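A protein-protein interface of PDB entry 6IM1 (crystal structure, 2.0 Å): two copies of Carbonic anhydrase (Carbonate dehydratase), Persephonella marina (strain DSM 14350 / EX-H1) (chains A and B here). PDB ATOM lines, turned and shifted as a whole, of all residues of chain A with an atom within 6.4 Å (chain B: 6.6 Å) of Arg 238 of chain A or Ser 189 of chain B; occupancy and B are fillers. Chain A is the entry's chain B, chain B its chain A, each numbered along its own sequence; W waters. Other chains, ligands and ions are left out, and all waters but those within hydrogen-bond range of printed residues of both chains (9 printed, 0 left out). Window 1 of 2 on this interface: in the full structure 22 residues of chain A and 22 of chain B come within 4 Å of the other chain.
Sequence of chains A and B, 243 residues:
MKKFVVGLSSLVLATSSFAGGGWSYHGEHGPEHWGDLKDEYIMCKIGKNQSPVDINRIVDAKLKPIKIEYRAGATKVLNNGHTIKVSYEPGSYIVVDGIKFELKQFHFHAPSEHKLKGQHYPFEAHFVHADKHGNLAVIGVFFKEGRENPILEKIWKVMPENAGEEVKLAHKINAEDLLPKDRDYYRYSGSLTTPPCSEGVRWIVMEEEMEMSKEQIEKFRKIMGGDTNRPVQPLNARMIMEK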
ATOM      1  N   LYS A  48     -15.996 -20.566  10.093  1.00  0.00           N
ATOM      2  CA  LYS A  48     -16.546 -20.155  11.397  1.00  0.00           C
ATOM      3  C   LYS A  48     -17.175 -21.299  12.210  1.00  0.00           C
ATOM      4  O   LYS A  48     -17.741 -21.080  13.316  1.00  0.00           O
ATOM      5  CB  LYS A  48     -17.613 -19.144  11.114  1.00  0.00           C
ATOM      6  CG  LYS A  48     -17.103 -17.890  10.375  1.00  0.00           C
ATOM      7  CD  LYS A  48     -16.211 -17.110  11.338  1.00  0.00           C
ATOM      8  CE  LYS A  48     -15.997 -15.688  10.855  1.00  0.00           C
ATOM      9  NZ  LYS A  48     -15.150 -14.965  11.823  1.00  0.00           N
ATOM     10  N   ASN A  49     -17.136 -22.520  11.682  1.00  0.00           N
ATOM     11  CA  ASN A  49     -17.615 -23.732  12.306  1.00  0.00           C
ATOM     12  C   ASN A  49     -16.598 -24.868  12.386  1.00  0.00           C
ATOM     13  O   ASN A  49     -16.843 -26.006  11.968  1.00  0.00           O
ATOM     14  CB  ASN A  49     -18.909 -24.217  11.618  1.00  0.00           C
ATOM     15  CG  ASN A  49     -20.026 -23.189  11.730  1.00  0.00           C
ATOM     16  OD1 ASN A  49     -20.756 -23.141  12.731  1.00  0.00           O
ATOM     17  ND2 ASN A  49     -20.135 -22.324  10.755  1.00  0.00           N
ATOM     18  N   GLN A  50     -15.449 -24.508  12.927  1.00  0.00           N
ATOM     19  CA  GLN A  50     -14.264 -25.386  12.938  1.00  0.00           C
ATOM     20  C   GLN A  50     -14.168 -26.125  14.241  1.00  0.00           C
ATOM     21  O   GLN A  50     -14.796 -25.764  15.282  1.00  0.00           O
ATOM     22  CB  GLN A  50     -13.003 -24.519  12.763  1.00  0.00           C
ATOM     23  CG  GLN A  50     -12.845 -23.853  11.420  1.00  0.00           C
ATOM     24  CD  GLN A  50     -12.395 -24.864  10.379  1.00  0.00           C
ATOM     25  OE1 GLN A  50     -11.255 -25.379  10.433  1.00  0.00           O
ATOM     26  NE2 GLN A  50     -13.282 -25.239   9.523  1.00  0.00           N
ATOM     27  N   SER A  51     -13.462 -27.240  14.166  1.00  0.00           N
ATOM     28  CA  SER A  51     -13.227 -28.124  15.294  1.00  0.00           C
ATOM     29  C   SER A  51     -11.670 -28.293  15.470  1.00  0.00           C
ATOM     30  O   SER A  51     -10.948 -28.091  14.513  1.00  0.00           O
ATOM     31  CB  SER A  51     -13.800 -29.461  15.007  1.00  0.00           C
ATOM     32  OG  SER A  51     -15.167 -29.442  14.855  1.00  0.00           O
ATOM     33  N   PRO A  52     -11.185 -28.648  16.660  1.00  0.00           N
ATOM     34  CA  PRO A  52     -12.025 -28.891  17.833  1.00  0.00           C
ATOM     35  C   PRO A  52     -12.380 -27.612  18.548  1.00  0.00           C
ATOM     36  O   PRO A  52     -12.004 -26.551  18.141  1.00  0.00           O
ATOM     37  CB  PRO A  52     -11.120 -29.738  18.704  1.00  0.00           C
ATOM     38  CG  PRO A  52      -9.726 -29.053  18.432  1.00  0.00           C
ATOM     39  CD  PRO A  52      -9.767 -28.748  16.982  1.00  0.00           C
ATOM     40  N   VAL A  53     -13.124 -27.746  19.615  1.00  0.00           N
ATOM     41  CA  VAL A  53     -13.532 -26.623  20.411  1.00  0.00           C
ATOM     42  C   VAL A  53     -13.423 -26.910  21.894  1.00  0.00           C
ATOM     43  O   VAL A  53     -13.283 -28.016  22.301  1.00  0.00           O
ATOM     44  CB  VAL A  53     -14.983 -26.181  20.106  1.00  0.00           C
ATOM     45  CG1 VAL A  53     -15.182 -25.863  18.658  1.00  0.00           C
ATOM     46  CG2 VAL A  53     -15.950 -27.241  20.532  1.00  0.00           C
ATOM     47  N   ARG A  57     -19.873 -23.931  26.398  1.00  0.00           N
ATOM     48  CA  ARG A  57     -21.133 -23.245  26.224  1.00  0.00           C
ATOM     49  C   ARG A  57     -22.101 -24.368  25.937  1.00  0.00           C
ATOM     50  O   ARG A  57     -22.297 -24.729  24.825  1.00  0.00           O
ATOM     51  CB  ARG A  57     -21.065 -22.245  25.082  1.00  0.00           C
ATOM     52  CG  ARG A  57     -22.319 -21.430  24.862  1.00  0.00           C
ATOM     53  CD  ARG A  57     -22.259 -20.714  23.535  1.00  0.00           C
ATOM     54  NE  ARG A  57     -21.477 -19.532  23.618  1.00  0.00           N
ATOM     55  CZ  ARG A  57     -20.912 -18.933  22.598  1.00  0.00           C
ATOM     56  NH1 ARG A  57     -21.011 -19.414  21.390  1.00  0.00           N
ATOM     57  NH2 ARG A  57     -20.237 -17.850  22.821  1.00  0.00           N
ATOM     58  N   TYR A 188     -22.367 -31.134  18.323  1.00  0.00           N
ATOM     59  CA  TYR A 188     -22.311 -29.839  17.647  1.00  0.00           C
ATOM     60  C   TYR A 188     -21.857 -30.066  16.176  1.00  0.00           C
ATOM     61  O   TYR A 188     -21.498 -31.179  15.792  1.00  0.00           O
ATOM     62  CB  TYR A 188     -21.331 -28.895  18.386  1.00  0.00           C
ATOM     63  CG  TYR A 188     -19.861 -29.175  18.236  1.00  0.00           C
ATOM     64  CD1 TYR A 188     -19.235 -30.148  18.950  1.00  0.00           C
ATOM     65  CD2 TYR A 188     -19.116 -28.484  17.273  1.00  0.00           C
ATOM     66  CE1 TYR A 188     -17.886 -30.448  18.743  1.00  0.00           C
ATOM     67  CE2 TYR A 188     -17.789 -28.768  17.051  1.00  0.00           C
ATOM     68  CZ  TYR A 188     -17.164 -29.715  17.794  1.00  0.00           C
ATOM     69  OH  TYR A 188     -15.816 -29.938  17.558  1.00  0.00           O
ATOM     70  N   SER A 189     -22.048 -29.031  15.381  1.00  0.00           N
ATOM     71  CA  SER A 189     -21.729 -28.986  13.970  1.00  0.00           C
ATOM     72  C   SER A 189     -20.332 -28.358  13.833  1.00  0.00           C
ATOM     73  O   SER A 189     -20.105 -27.227  14.261  1.00  0.00           O
ATOM     74  CB  SER A 189     -22.715 -28.136  13.218  1.00  0.00           C
ATOM     75  OG  SER A 189     -22.357 -27.895  11.863  1.00  0.00           O
ATOM     76  N   GLY A 190     -19.440 -29.108  13.250  1.00  0.00           N
ATOM     77  CA  GLY A 190     -18.090 -28.713  13.145  1.00  0.00           C
ATOM     78  C   GLY A 190     -17.374 -29.174  11.888  1.00  0.00           C
ATOM     79  O   GLY A 190     -17.920 -29.162  10.806  1.00  0.00           O
ATOM     80  N   SER A 191     -16.099 -29.528  12.072  1.00  0.00           N
ATOM     81  CA  SER A 191     -15.168 -29.718  10.914  1.00  0.00           C
ATOM     82  C   SER A 191     -14.231 -30.882  11.156  1.00  0.00           C
ATOM     83  O   SER A 191     -14.076 -31.374  12.285  1.00  0.00           O
ATOM     84  CB  SER A 191     -14.301 -28.456  10.643  1.00  0.00           C
ATOM     85  OG  SER A 191     -13.205 -28.316  11.535  1.00  0.00           O
ATOM     86  N   GLN A 233     -10.732 -24.032  18.476  1.00  0.00           N
ATOM     87  CA  GLN A 233     -11.191 -22.999  17.571  1.00  0.00           C
ATOM     88  C   GLN A 233     -12.453 -22.355  18.185  1.00  0.00           C
ATOM     89  O   GLN A 233     -13.165 -23.010  18.966  1.00  0.00           O
ATOM     90  CB  GLN A 233     -11.577 -23.645  16.231  1.00  0.00           C
ATOM     91  CG  GLN A 233     -10.445 -24.424  15.561  1.00  0.00           C
ATOM     92  CD  GLN A 233      -9.354 -23.484  15.114  1.00  0.00           C
ATOM     93  OE1 GLN A 233      -9.645 -22.471  14.504  1.00  0.00           O
ATOM     94  NE2 GLN A 233      -8.117 -23.709  15.594  1.00  0.00           N
ATOM     95  N   PRO A 234     -12.736 -21.112  17.834  1.00  0.00           N
ATOM     96  CA  PRO A 234     -13.832 -20.433  18.506  1.00  0.00           C
ATOM     97  C   PRO A 234     -15.178 -21.086  18.178  1.00  0.00           C
ATOM     98  O   PRO A 234     -15.446 -21.452  17.003  1.00  0.00           O
ATOM     99  CB  PRO A 234     -13.775 -19.010  17.899  1.00  0.00           C
ATOM    100  CG  PRO A 234     -12.416 -18.865  17.308  1.00  0.00           C
ATOM    101  CD  PRO A 234     -12.004 -20.226  16.890  1.00  0.00           C
ATOM    102  N   LEU A 235     -16.084 -21.038  19.134  1.00  0.00           N
ATOM    103  CA  LEU A 235     -17.426 -21.533  18.958  1.00  0.00           C
ATOM    104  C   LEU A 235     -18.222 -20.687  17.988  1.00  0.00           C
ATOM    105  O   LEU A 235     -19.032 -21.178  17.256  1.00  0.00           O
ATOM    106  CB  LEU A 235     -18.144 -21.593  20.281  1.00  0.00           C
ATOM    107  CG  LEU A 235     -17.945 -22.866  21.059  1.00  0.00           C
ATOM    108  CD1 LEU A 235     -18.567 -22.742  22.423  1.00  0.00           C
ATOM    109  CD2 LEU A 235     -18.536 -24.012  20.294  1.00  0.00           C
ATOM    110  N   ASN A 236     -17.980 -19.397  18.040  1.00  0.00           N
ATOM    111  CA  ASN A 236     -18.673 -18.444  17.224  1.00  0.00           C
ATOM    112  C   ASN A 236     -20.171 -18.469  17.541  1.00  0.00           C
ATOM    113  O   ASN A 236     -20.540 -18.236  18.641  1.00  0.00           O
ATOM    114  CB  ASN A 236     -18.323 -18.610  15.756  1.00  0.00           C
ATOM    115  CG  ASN A 236     -16.869 -18.280  15.456  1.00  0.00           C
ATOM    116  OD1 ASN A 236     -16.212 -18.980  14.739  1.00  0.00           O
ATOM    117  ND2 ASN A 236     -16.388 -17.226  16.018  1.00  0.00           N
ATOM    118  N   ALA A 237     -21.011 -18.723  16.562  1.00  0.00           N
ATOM    119  CA  ALA A 237     -22.439 -18.761  16.772  1.00  0.00           C
ATOM    120  C   ALA A 237     -22.977 -20.012  17.437  1.00  0.00           C
ATOM    121  O   ALA A 237     -24.090 -20.046  17.815  1.00  0.00           O
ATOM    122  CB  ALA A 237     -23.159 -18.529  15.466  1.00  0.00           C
ATOM    123  N   ARG A 238     -22.155 -21.066  17.612  1.00  0.00           N
ATOM    124  CA  ARG A 238     -22.599 -22.371  18.048  1.00  0.00           C
ATOM    125  C   ARG A 238     -22.829 -22.517  19.523  1.00  0.00           C
ATOM    126  O   ARG A 238     -22.193 -21.868  20.323  1.00  0.00           O
ATOM    127  CB  ARG A 238     -21.569 -23.428  17.592  1.00  0.00           C
ATOM    128  CG  ARG A 238     -21.454 -23.502  16.053  1.00  0.00           C
ATOM    129  CD  ARG A 238     -20.322 -24.478  15.699  1.00  0.00           C
ATOM    130  NE  ARG A 238     -19.021 -23.882  15.952  1.00  0.00           N
ATOM    131  CZ  ARG A 238     -17.858 -24.463  15.721  1.00  0.00           C
ATOM    132  NH1 ARG A 238     -17.838 -25.727  15.279  1.00  0.00           N
ATOM    133  NH2 ARG A 238     -16.724 -23.833  16.021  1.00  0.00           N
ATOM    134  N   MET A 239     -23.751 -23.422  19.840  1.00  0.00           N
ATOM    135  CA  MET A 239     -23.875 -23.982  21.192  1.00  0.00           C
ATOM    136  C   MET A 239     -23.591 -25.469  21.138  1.00  0.00           C
ATOM    137  O   MET A 239     -23.635 -26.056  20.097  1.00  0.00           O
ATOM    138  CB  MET A 239     -25.324 -23.851  21.645  1.00  0.00           C
ATOM    139  CG  MET A 239     -25.749 -22.432  21.695  1.00  0.00           C
ATOM    140  SD  MET A 239     -26.992 -22.202  22.962  1.00  0.00           S
ATOM    141  CE  MET A 239     -25.853 -22.520  24.349  1.00  0.00           C
ATOM    142  N   ILE A 240     -23.134 -26.044  22.238  1.00  0.00           N
ATOM    143  CA  ILE A 240     -22.923 -27.479  22.263  1.00  0.00           C
ATOM    144  C   ILE A 240     -24.188 -28.046  22.988  1.00  0.00           C
ATOM    145  O   ILE A 240     -24.560 -27.506  24.057  1.00  0.00           O
ATOM    146  CB  ILE A 240     -21.676 -27.820  23.051  1.00  0.00           C
ATOM    147  CG1 ILE A 240     -20.423 -27.018  22.670  1.00  0.00           C
ATOM    148  CG2 ILE A 240     -21.501 -29.321  23.019  1.00  0.00           C
ATOM    149  CD1 ILE A 240     -20.125 -27.182  21.283  1.00  0.00           C
ATOM    150  N   ASN B  49     -22.992 -24.354   6.461  1.00  0.00           N
ATOM    151  CA  ASN B  49     -23.776 -23.806   7.536  1.00  0.00           C
ATOM    152  C   ASN B  49     -24.509 -22.544   7.039  1.00  0.00           C
ATOM    153  O   ASN B  49     -24.448 -21.521   7.619  1.00  0.00           O
ATOM    154  CB  ASN B  49     -22.883 -23.535   8.750  1.00  0.00           C
ATOM    155  CG  ASN B  49     -22.271 -24.804   9.327  1.00  0.00           C
ATOM    156  OD1 ASN B  49     -22.905 -25.522  10.045  1.00  0.00           O
ATOM    157  ND2 ASN B  49     -21.045 -25.082   8.968  1.00  0.00           N
ATOM    158  N   GLN B  50     -25.167 -22.690   5.918  1.00  0.00           N
ATOM    159  CA  GLN B  50     -25.897 -21.633   5.267  1.00  0.00           C
ATOM    160  C   GLN B  50     -27.336 -21.444   5.765  1.00  0.00           C
ATOM    161  O   GLN B  50     -27.903 -22.327   6.310  1.00  0.00           O
ATOM    162  CB  GLN B  50     -25.859 -21.845   3.760  1.00  0.00           C
ATOM    163  CG  GLN B  50     -24.486 -21.715   3.138  1.00  0.00           C
ATOM    164  CD  GLN B  50     -24.032 -20.290   3.014  1.00  0.00           C
ATOM    165  OE1 GLN B  50     -24.487 -19.567   2.184  1.00  0.00           O
ATOM    166  NE2 GLN B  50     -23.139 -19.891   3.861  1.00  0.00           N
ATOM    167  N   SER B  51     -27.876 -20.269   5.526  1.00  0.00           N
ATOM    168  CA  SER B  51     -29.223 -19.872   5.863  1.00  0.00           C
ATOM    169  C   SER B  51     -29.840 -19.326   4.574  1.00  0.00           C
ATOM    170  O   SER B  51     -29.125 -18.892   3.746  1.00  0.00           O
ATOM    171  CB  SER B  51     -29.214 -18.788   6.925  1.00  0.00           C
ATOM    172  OG  SER B  51     -28.657 -19.242   8.088  1.00  0.00           O
ATOM    173  N   ASP B  97     -25.797 -15.335  24.629  1.00  0.00           N
ATOM    174  CA  ASP B  97     -24.569 -15.903  25.223  1.00  0.00           C
ATOM    175  C   ASP B  97     -23.774 -14.929  26.102  1.00  0.00           C
ATOM    176  O   ASP B  97     -22.533 -14.863  26.037  1.00  0.00           O
ATOM    177  CB  ASP B  97     -23.670 -16.364  24.056  1.00  0.00           C
ATOM    178  CG  ASP B  97     -24.339 -17.449  23.167  1.00  0.00           C
ATOM    179  OD1 ASP B  97     -25.211 -18.213  23.696  1.00  0.00           O
ATOM    180  OD2 ASP B  97     -23.967 -17.567  21.972  1.00  0.00           O
ATOM    181  N   ARG B 187     -33.188 -21.660  17.610  1.00  0.00           N
ATOM    182  CA  ARG B 187     -31.834 -21.183  17.452  1.00  0.00           C
ATOM    183  C   ARG B 187     -30.957 -22.107  16.702  1.00  0.00           C
ATOM    184  O   ARG B 187     -31.017 -23.329  16.883  1.00  0.00           O
ATOM    185  CB  ARG B 187     -31.177 -20.837  18.799  1.00  0.00           C
ATOM    186  CG  ARG B 187     -29.711 -20.490  18.706  1.00  0.00           C
ATOM    187  CD  ARG B 187     -29.092 -20.078  20.002  1.00  0.00           C
ATOM    188  NE  ARG B 187     -27.687 -19.950  19.843  1.00  0.00           N
ATOM    189  CZ  ARG B 187     -26.850 -19.386  20.695  1.00  0.00           C
ATOM    190  NH1 ARG B 187     -27.276 -18.955  21.884  1.00  0.00           N
ATOM    191  NH2 ARG B 187     -25.543 -19.321  20.380  1.00  0.00           N
ATOM    192  N   TYR B 188     -30.148 -21.536  15.797  1.00  0.00           N
ATOM    193  CA  TYR B 188     -29.128 -22.347  15.074  1.00  0.00           C
ATOM    194  C   TYR B 188     -28.021 -21.408  14.549  1.00  0.00           C
ATOM    195  O   TYR B 188     -28.150 -20.182  14.617  1.00  0.00           O
ATOM    196  CB  TYR B 188     -29.757 -23.131  13.909  1.00  0.00           C
ATOM    197  CG  TYR B 188     -30.132 -22.325  12.656  1.00  0.00           C
ATOM    198  CD1 TYR B 188     -31.298 -21.630  12.599  1.00  0.00           C
ATOM    199  CD2 TYR B 188     -29.271 -22.237  11.606  1.00  0.00           C
ATOM    200  CE1 TYR B 188     -31.633 -20.903  11.487  1.00  0.00           C
ATOM    201  CE2 TYR B 188     -29.585 -21.557  10.475  1.00  0.00           C
ATOM    202  CZ  TYR B 188     -30.777 -20.834  10.424  1.00  0.00           C
ATOM    203  OH  TYR B 188     -31.053 -20.128   9.302  1.00  0.00           O
ATOM    204  N   SER B 189     -26.931 -22.027  14.154  1.00  0.00           N
ATOM    205  CA  SER B 189     -25.770 -21.376  13.629  1.00  0.00           C
ATOM    206  C   SER B 189     -25.780 -21.399  12.097  1.00  0.00           C
ATOM    207  O   SER B 189     -25.923 -22.454  11.505  1.00  0.00           O
ATOM    208  CB  SER B 189     -24.496 -22.118  14.082  1.00  0.00           C
ATOM    209  OG  SER B 189     -23.318 -21.634  13.413  1.00  0.00           O
ATOM    210  N   GLY B 190     -25.808 -20.213  11.516  1.00  0.00           N
ATOM    211  CA  GLY B 190     -26.001 -20.059  10.117  1.00  0.00           C
ATOM    212  C   GLY B 190     -25.248 -18.963   9.457  1.00  0.00           C
ATOM    213  O   GLY B 190     -24.106 -18.669   9.819  1.00  0.00           O
ATOM    214  N   SER B 191     -25.933 -18.278   8.513  1.00  0.00           N
ATOM    215  CA  SER B 191     -25.232 -17.341   7.608  1.00  0.00           C
ATOM    216  C   SER B 191     -26.092 -16.158   7.294  1.00  0.00           C
ATOM    217  O   SER B 191     -27.315 -16.153   7.528  1.00  0.00           O
ATOM    218  CB  SER B 191     -24.830 -17.994   6.261  1.00  0.00           C
ATOM    219  OG  SER B 191     -25.903 -18.155   5.363  1.00  0.00           O
ATOM    220  N   GLU B 199     -20.707 -16.877   7.225  1.00  0.00           N
ATOM    221  CA  GLU B 199     -21.131 -17.779   8.316  1.00  0.00           C
ATOM    222  C   GLU B 199     -20.803 -17.224   9.685  1.00  0.00           C
ATOM    223  O   GLU B 199     -20.313 -16.096   9.821  1.00  0.00           O
ATOM    224  CB  GLU B 199     -20.625 -19.208   8.044  1.00  0.00           C
ATOM    225  CG  GLU B 199     -21.405 -19.803   6.854  1.00  0.00           C
ATOM    226  CD  GLU B 199     -21.062 -21.240   6.538  1.00  0.00           C
ATOM    227  OE1 GLU B 199     -20.239 -21.858   7.249  1.00  0.00           O
ATOM    228  OE2 GLU B 199     -21.750 -21.816   5.613  1.00  0.00           O
ATOM    229  N   GLY B 200     -21.094 -17.975  10.718  1.00  0.00           N
ATOM    230  CA  GLY B 200     -20.809 -17.497  12.055  1.00  0.00           C
ATOM    231  C   GLY B 200     -21.930 -16.610  12.551  1.00  0.00           C
ATOM    232  O   GLY B 200     -21.769 -15.859  13.487  1.00  0.00           O
ATOM    233  N   VAL B 201     -23.107 -16.737  11.959  1.00  0.00           N
ATOM    234  CA  VAL B 201     -24.260 -15.868  12.339  1.00  0.00           C
ATOM    235  C   VAL B 201     -25.160 -16.612  13.316  1.00  0.00           C
ATOM    236  O   VAL B 201     -25.580 -17.734  13.017  1.00  0.00           O
ATOM    237  CB  VAL B 201     -25.047 -15.465  11.097  1.00  0.00           C
ATOM    238  CG1 VAL B 201     -26.296 -14.590  11.448  1.00  0.00           C
ATOM    239  CG2 VAL B 201     -24.143 -14.688  10.191  1.00  0.00           C
ATOM    240  N   ARG B 202     -25.508 -15.966  14.438  1.00  0.00           N
ATOM    241  CA  ARG B 202     -26.514 -16.471  15.353  1.00  0.00           C
ATOM    242  C   ARG B 202     -27.903 -16.216  14.851  1.00  0.00           C
ATOM    243  O   ARG B 202     -28.247 -15.052  14.694  1.00  0.00           O
ATOM    244  CB  ARG B 202     -26.353 -15.926  16.750  1.00  0.00           C
ATOM    245  CG  ARG B 202     -25.042 -16.395  17.445  1.00  0.00           C
ATOM    246  CD  ARG B 202     -24.775 -15.425  18.614  1.00  0.00           C
ATOM    247  NE  ARG B 202     -23.847 -15.881  19.633  1.00  0.00           N
ATOM    248  CZ  ARG B 202     -22.524 -15.679  19.594  1.00  0.00           C
ATOM    249  NH1 ARG B 202     -21.964 -15.136  18.539  1.00  0.00           N
ATOM    250  NH2 ARG B 202     -21.755 -16.193  20.581  1.00  0.00           N
ATOM    251  N   TRP B 203     -28.670 -17.249  14.577  1.00  0.00           N
ATOM    252  CA  TRP B 203     -30.049 -17.110  14.192  1.00  0.00           C
ATOM    253  C   TRP B 203     -30.999 -17.431  15.304  1.00  0.00           C
ATOM    254  O   TRP B 203     -30.904 -18.461  15.969  1.00  0.00           O
ATOM    255  CB  TRP B 203     -30.420 -17.979  12.955  1.00  0.00           C
ATOM    256  CG  TRP B 203     -30.039 -17.361  11.697  1.00  0.00           C
ATOM    257  CD1 TRP B 203     -28.864 -17.534  11.006  1.00  0.00           C
ATOM    258  CD2 TRP B 203     -30.787 -16.384  10.979  1.00  0.00           C
ATOM    259  NE1 TRP B 203     -28.877 -16.762   9.893  1.00  0.00           N
ATOM    260  CE2 TRP B 203     -29.994 -15.988   9.873  1.00  0.00           C
ATOM    261  CE3 TRP B 203     -32.025 -15.820  11.159  1.00  0.00           C
ATOM    262  CZ2 TRP B 203     -30.441 -15.082   8.928  1.00  0.00           C
ATOM    263  CZ3 TRP B 203     -32.473 -14.898  10.264  1.00  0.00           C
ATOM    264  CH2 TRP B 203     -31.699 -14.578   9.134  1.00  0.00           C
ATOM    265  N   ARG B 238     -26.290 -29.747  11.230  1.00  0.00           N
ATOM    266  CA  ARG B 238     -26.944 -28.948  12.266  1.00  0.00           C
ATOM    267  C   ARG B 238     -28.260 -29.548  12.752  1.00  0.00           C
ATOM    268  O   ARG B 238     -28.951 -30.210  12.045  1.00  0.00           O
ATOM    269  CB  ARG B 238     -27.172 -27.501  11.704  1.00  0.00           C
ATOM    270  CG  ARG B 238     -25.886 -26.770  11.373  1.00  0.00           C
ATOM    271  CD  ARG B 238     -26.207 -25.469  10.730  1.00  0.00           C
ATOM    272  NE  ARG B 238     -26.712 -25.644   9.371  1.00  0.00           N
ATOM    273  CZ  ARG B 238     -27.082 -24.684   8.548  1.00  0.00           C
ATOM    274  NH1 ARG B 238     -27.013 -23.418   8.936  1.00  0.00           N
ATOM    275  NH2 ARG B 238     -27.443 -24.975   7.317  1.00  0.00           N
ATOM    276  N   MET B 239     -28.573 -29.237  14.005  1.00  0.00           N
ATOM    277  CA  MET B 239     -29.905 -29.369  14.569  1.00  0.00           C
ATOM    278  C   MET B 239     -30.434 -27.949  14.908  1.00  0.00           C
ATOM    279  O   MET B 239     -29.673 -27.020  15.034  1.00  0.00           O
ATOM    280  CB  MET B 239     -29.829 -30.097  15.856  1.00  0.00           C
ATOM    281  CG  MET B 239     -29.281 -31.459  15.662  1.00  0.00           C
ATOM    282  SD  MET B 239     -29.984 -32.567  16.878  1.00  0.00           S
ATOM    283  CE  MET B 239     -31.664 -32.513  16.213  1.00  0.00           C
ATOM    284  N   ILE B 240     -31.731 -27.805  14.971  1.00  0.00           N
ATOM    285  CA  ILE B 240     -32.325 -26.513  15.356  1.00  0.00           C
ATOM    286  C   ILE B 240     -32.782 -26.731  16.818  1.00  0.00           C
ATOM    287  O   ILE B 240     -33.425 -27.743  17.088  1.00  0.00           O
ATOM    288  CB  ILE B 240     -33.502 -26.135  14.513  1.00  0.00           C
ATOM    289  CG1 ILE B 240     -33.290 -26.238  12.989  1.00  0.00           C
ATOM    290  CG2 ILE B 240     -34.034 -24.796  14.959  1.00  0.00           C
ATOM    291  CD1 ILE B 240     -32.182 -25.399  12.558  1.00  0.00           C
ATOM    292  N   MET B 241     -32.386 -25.875  17.712  1.00  0.00           N
ATOM    293  CA  MET B 241     -32.756 -25.945  19.077  1.00  0.00           C
ATOM    294  C   MET B 241     -33.997 -25.086  19.298  1.00  0.00           C
ATOM    295  O   MET B 241     -34.122 -23.997  18.760  1.00  0.00           O
ATOM    296  CB  MET B 241     -31.676 -25.437  19.979  1.00  0.00           C
ATOM    297  CG  MET B 241     -30.422 -26.320  19.904  1.00  0.00           C
ATOM    298  SD  MET B 241     -29.056 -25.533  20.780  1.00  0.00           S
ATOM    299  CE  MET B 241     -28.709 -24.103  19.746  1.00  0.00           C
HETATM  300  O   HOH W   1     -20.499 -20.342  14.007  1.00  0.00           O
HETATM  301  O   HOH W   2     -22.505 -20.484  10.914  1.00  0.00           O
HETATM  302  O   HOH W   3     -18.803 -16.503  20.792  1.00  0.00           O
HETATM  303  O   HOH W   4     -20.311 -16.402  25.254  1.00  0.00           O
HETATM  304  O   HOH W   5     -23.348 -28.316   8.922  1.00  0.00           O
HETATM  305  O   HOH W   6     -17.983 -21.583   8.484  1.00  0.00           O
HETATM  306  O   HOH W   7     -20.025 -27.527  10.314  1.00  0.00           O
HETATM  307  O   HOH W   8     -26.546 -21.587  17.662  1.00  0.00           O
HETATM  308  O   HOH W   9     -23.017 -24.729  12.854  1.00  0.00           O
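The side-chain amide oxygen of Asn 49 of chain A is in hydrogen-bond range of the side-chain hydroxyl of Ser 189 of chain B (3.0 Å). The guanidinium group (NH1) of Arg 57 of chain A lies within salt-bridge range of the side-chain carboxylate (OD2) of Asp 97 of chain B (3.5 Å). The guanidinium group of Arg 202 of chain B sits at hydrogen-bond distance from the backbone carbonyl oxygen of Asn 236 of chain A. The side-chain sulfur of Met 239 of chain A lies within hydrogen-bond range of the guanidinium group of Arg 187 of chain B (3.4 Å). NH2 of Arg 187 of chain B is in hydrogen-bond range of O of Ala 237 of chain A, 3.0 Å away. The side-chain amide oxygen of Asn 49 of chain B sits at hydrogen-bond distance from the side-chain hydroxyl of Ser 189 of chain A (3.0 Å). The guanidinium group of Arg 57 of chain A lies close to the guanidinium group of Arg 202 of chain B (3.2 Å).
O of Asn 49 of chain B sits close to NH1 of Arg 238 of chain B (3.5 Å). The backbone carbonyl oxygen of Gln 50 of chain B is in hydrogen-bond range of the guanidinium group of Arg 238 of chain B.
O of Glu 199 of chain B touches CG of Lys 48 of chain A, at 3.7 Å. Asn 49 of chain A touches Glu 199 of chain B. Gly 200 of chain B touches Ala 237 of chain A (O to CB, 3.6 Å). Ala 237 of chain A touches Val 201 of chain B (CB to C, 3.5 Å).
Arg 238 of chain A touches one residue of chain B. Ser 189 of chain B touches just these residues of chain A: Asn 49 (3.0 Å), Ala 237 (3.7 Å) and Arg 238 (3.7 Å). Of the printed residues of chain B, Arg 57 of chain A touches Asp 97 (3.4 Å) and Arg 202 (3.2 Å). Of the printed residues of chain B, Ala 237 of chain A touches Arg 187, Ser 189, Gly 200, Val 201 and Arg 202.
Of the 19 printed residues of chain A, 8 touch a printed residue of chain B. Hydrophobic or aromatic side chains of chain A that line the printed part of chain B: Ala 237 and Met 239. Printed residues of chain B that touch a printed residue of chain A: Asn 49, Asp 97, Arg 187, Ser 189, Glu 199, Gly 200, Val 201, Arg 202, Arg 238 and Met 241. Hydrophobic or aromatic side chains of chain B within 4 Å of the printed part of chain A: Met 241. Along chain B the printed residues that touch a printed residue of chain A span positions 49 to 241.
Asn 49 of chain A touches its own counterpart, Asn 49 of chain B. Ser 189 of chain A touches Arg 238 of chain B, and with the chains exchanged Arg 238 of chain A touches Ser 189 of chain B.
Water W5 bridges the side-chain amide oxygen (OD1) of Asn 49 of chain B and the side-chain hydroxyl (OG) of Ser 189 of chain A.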
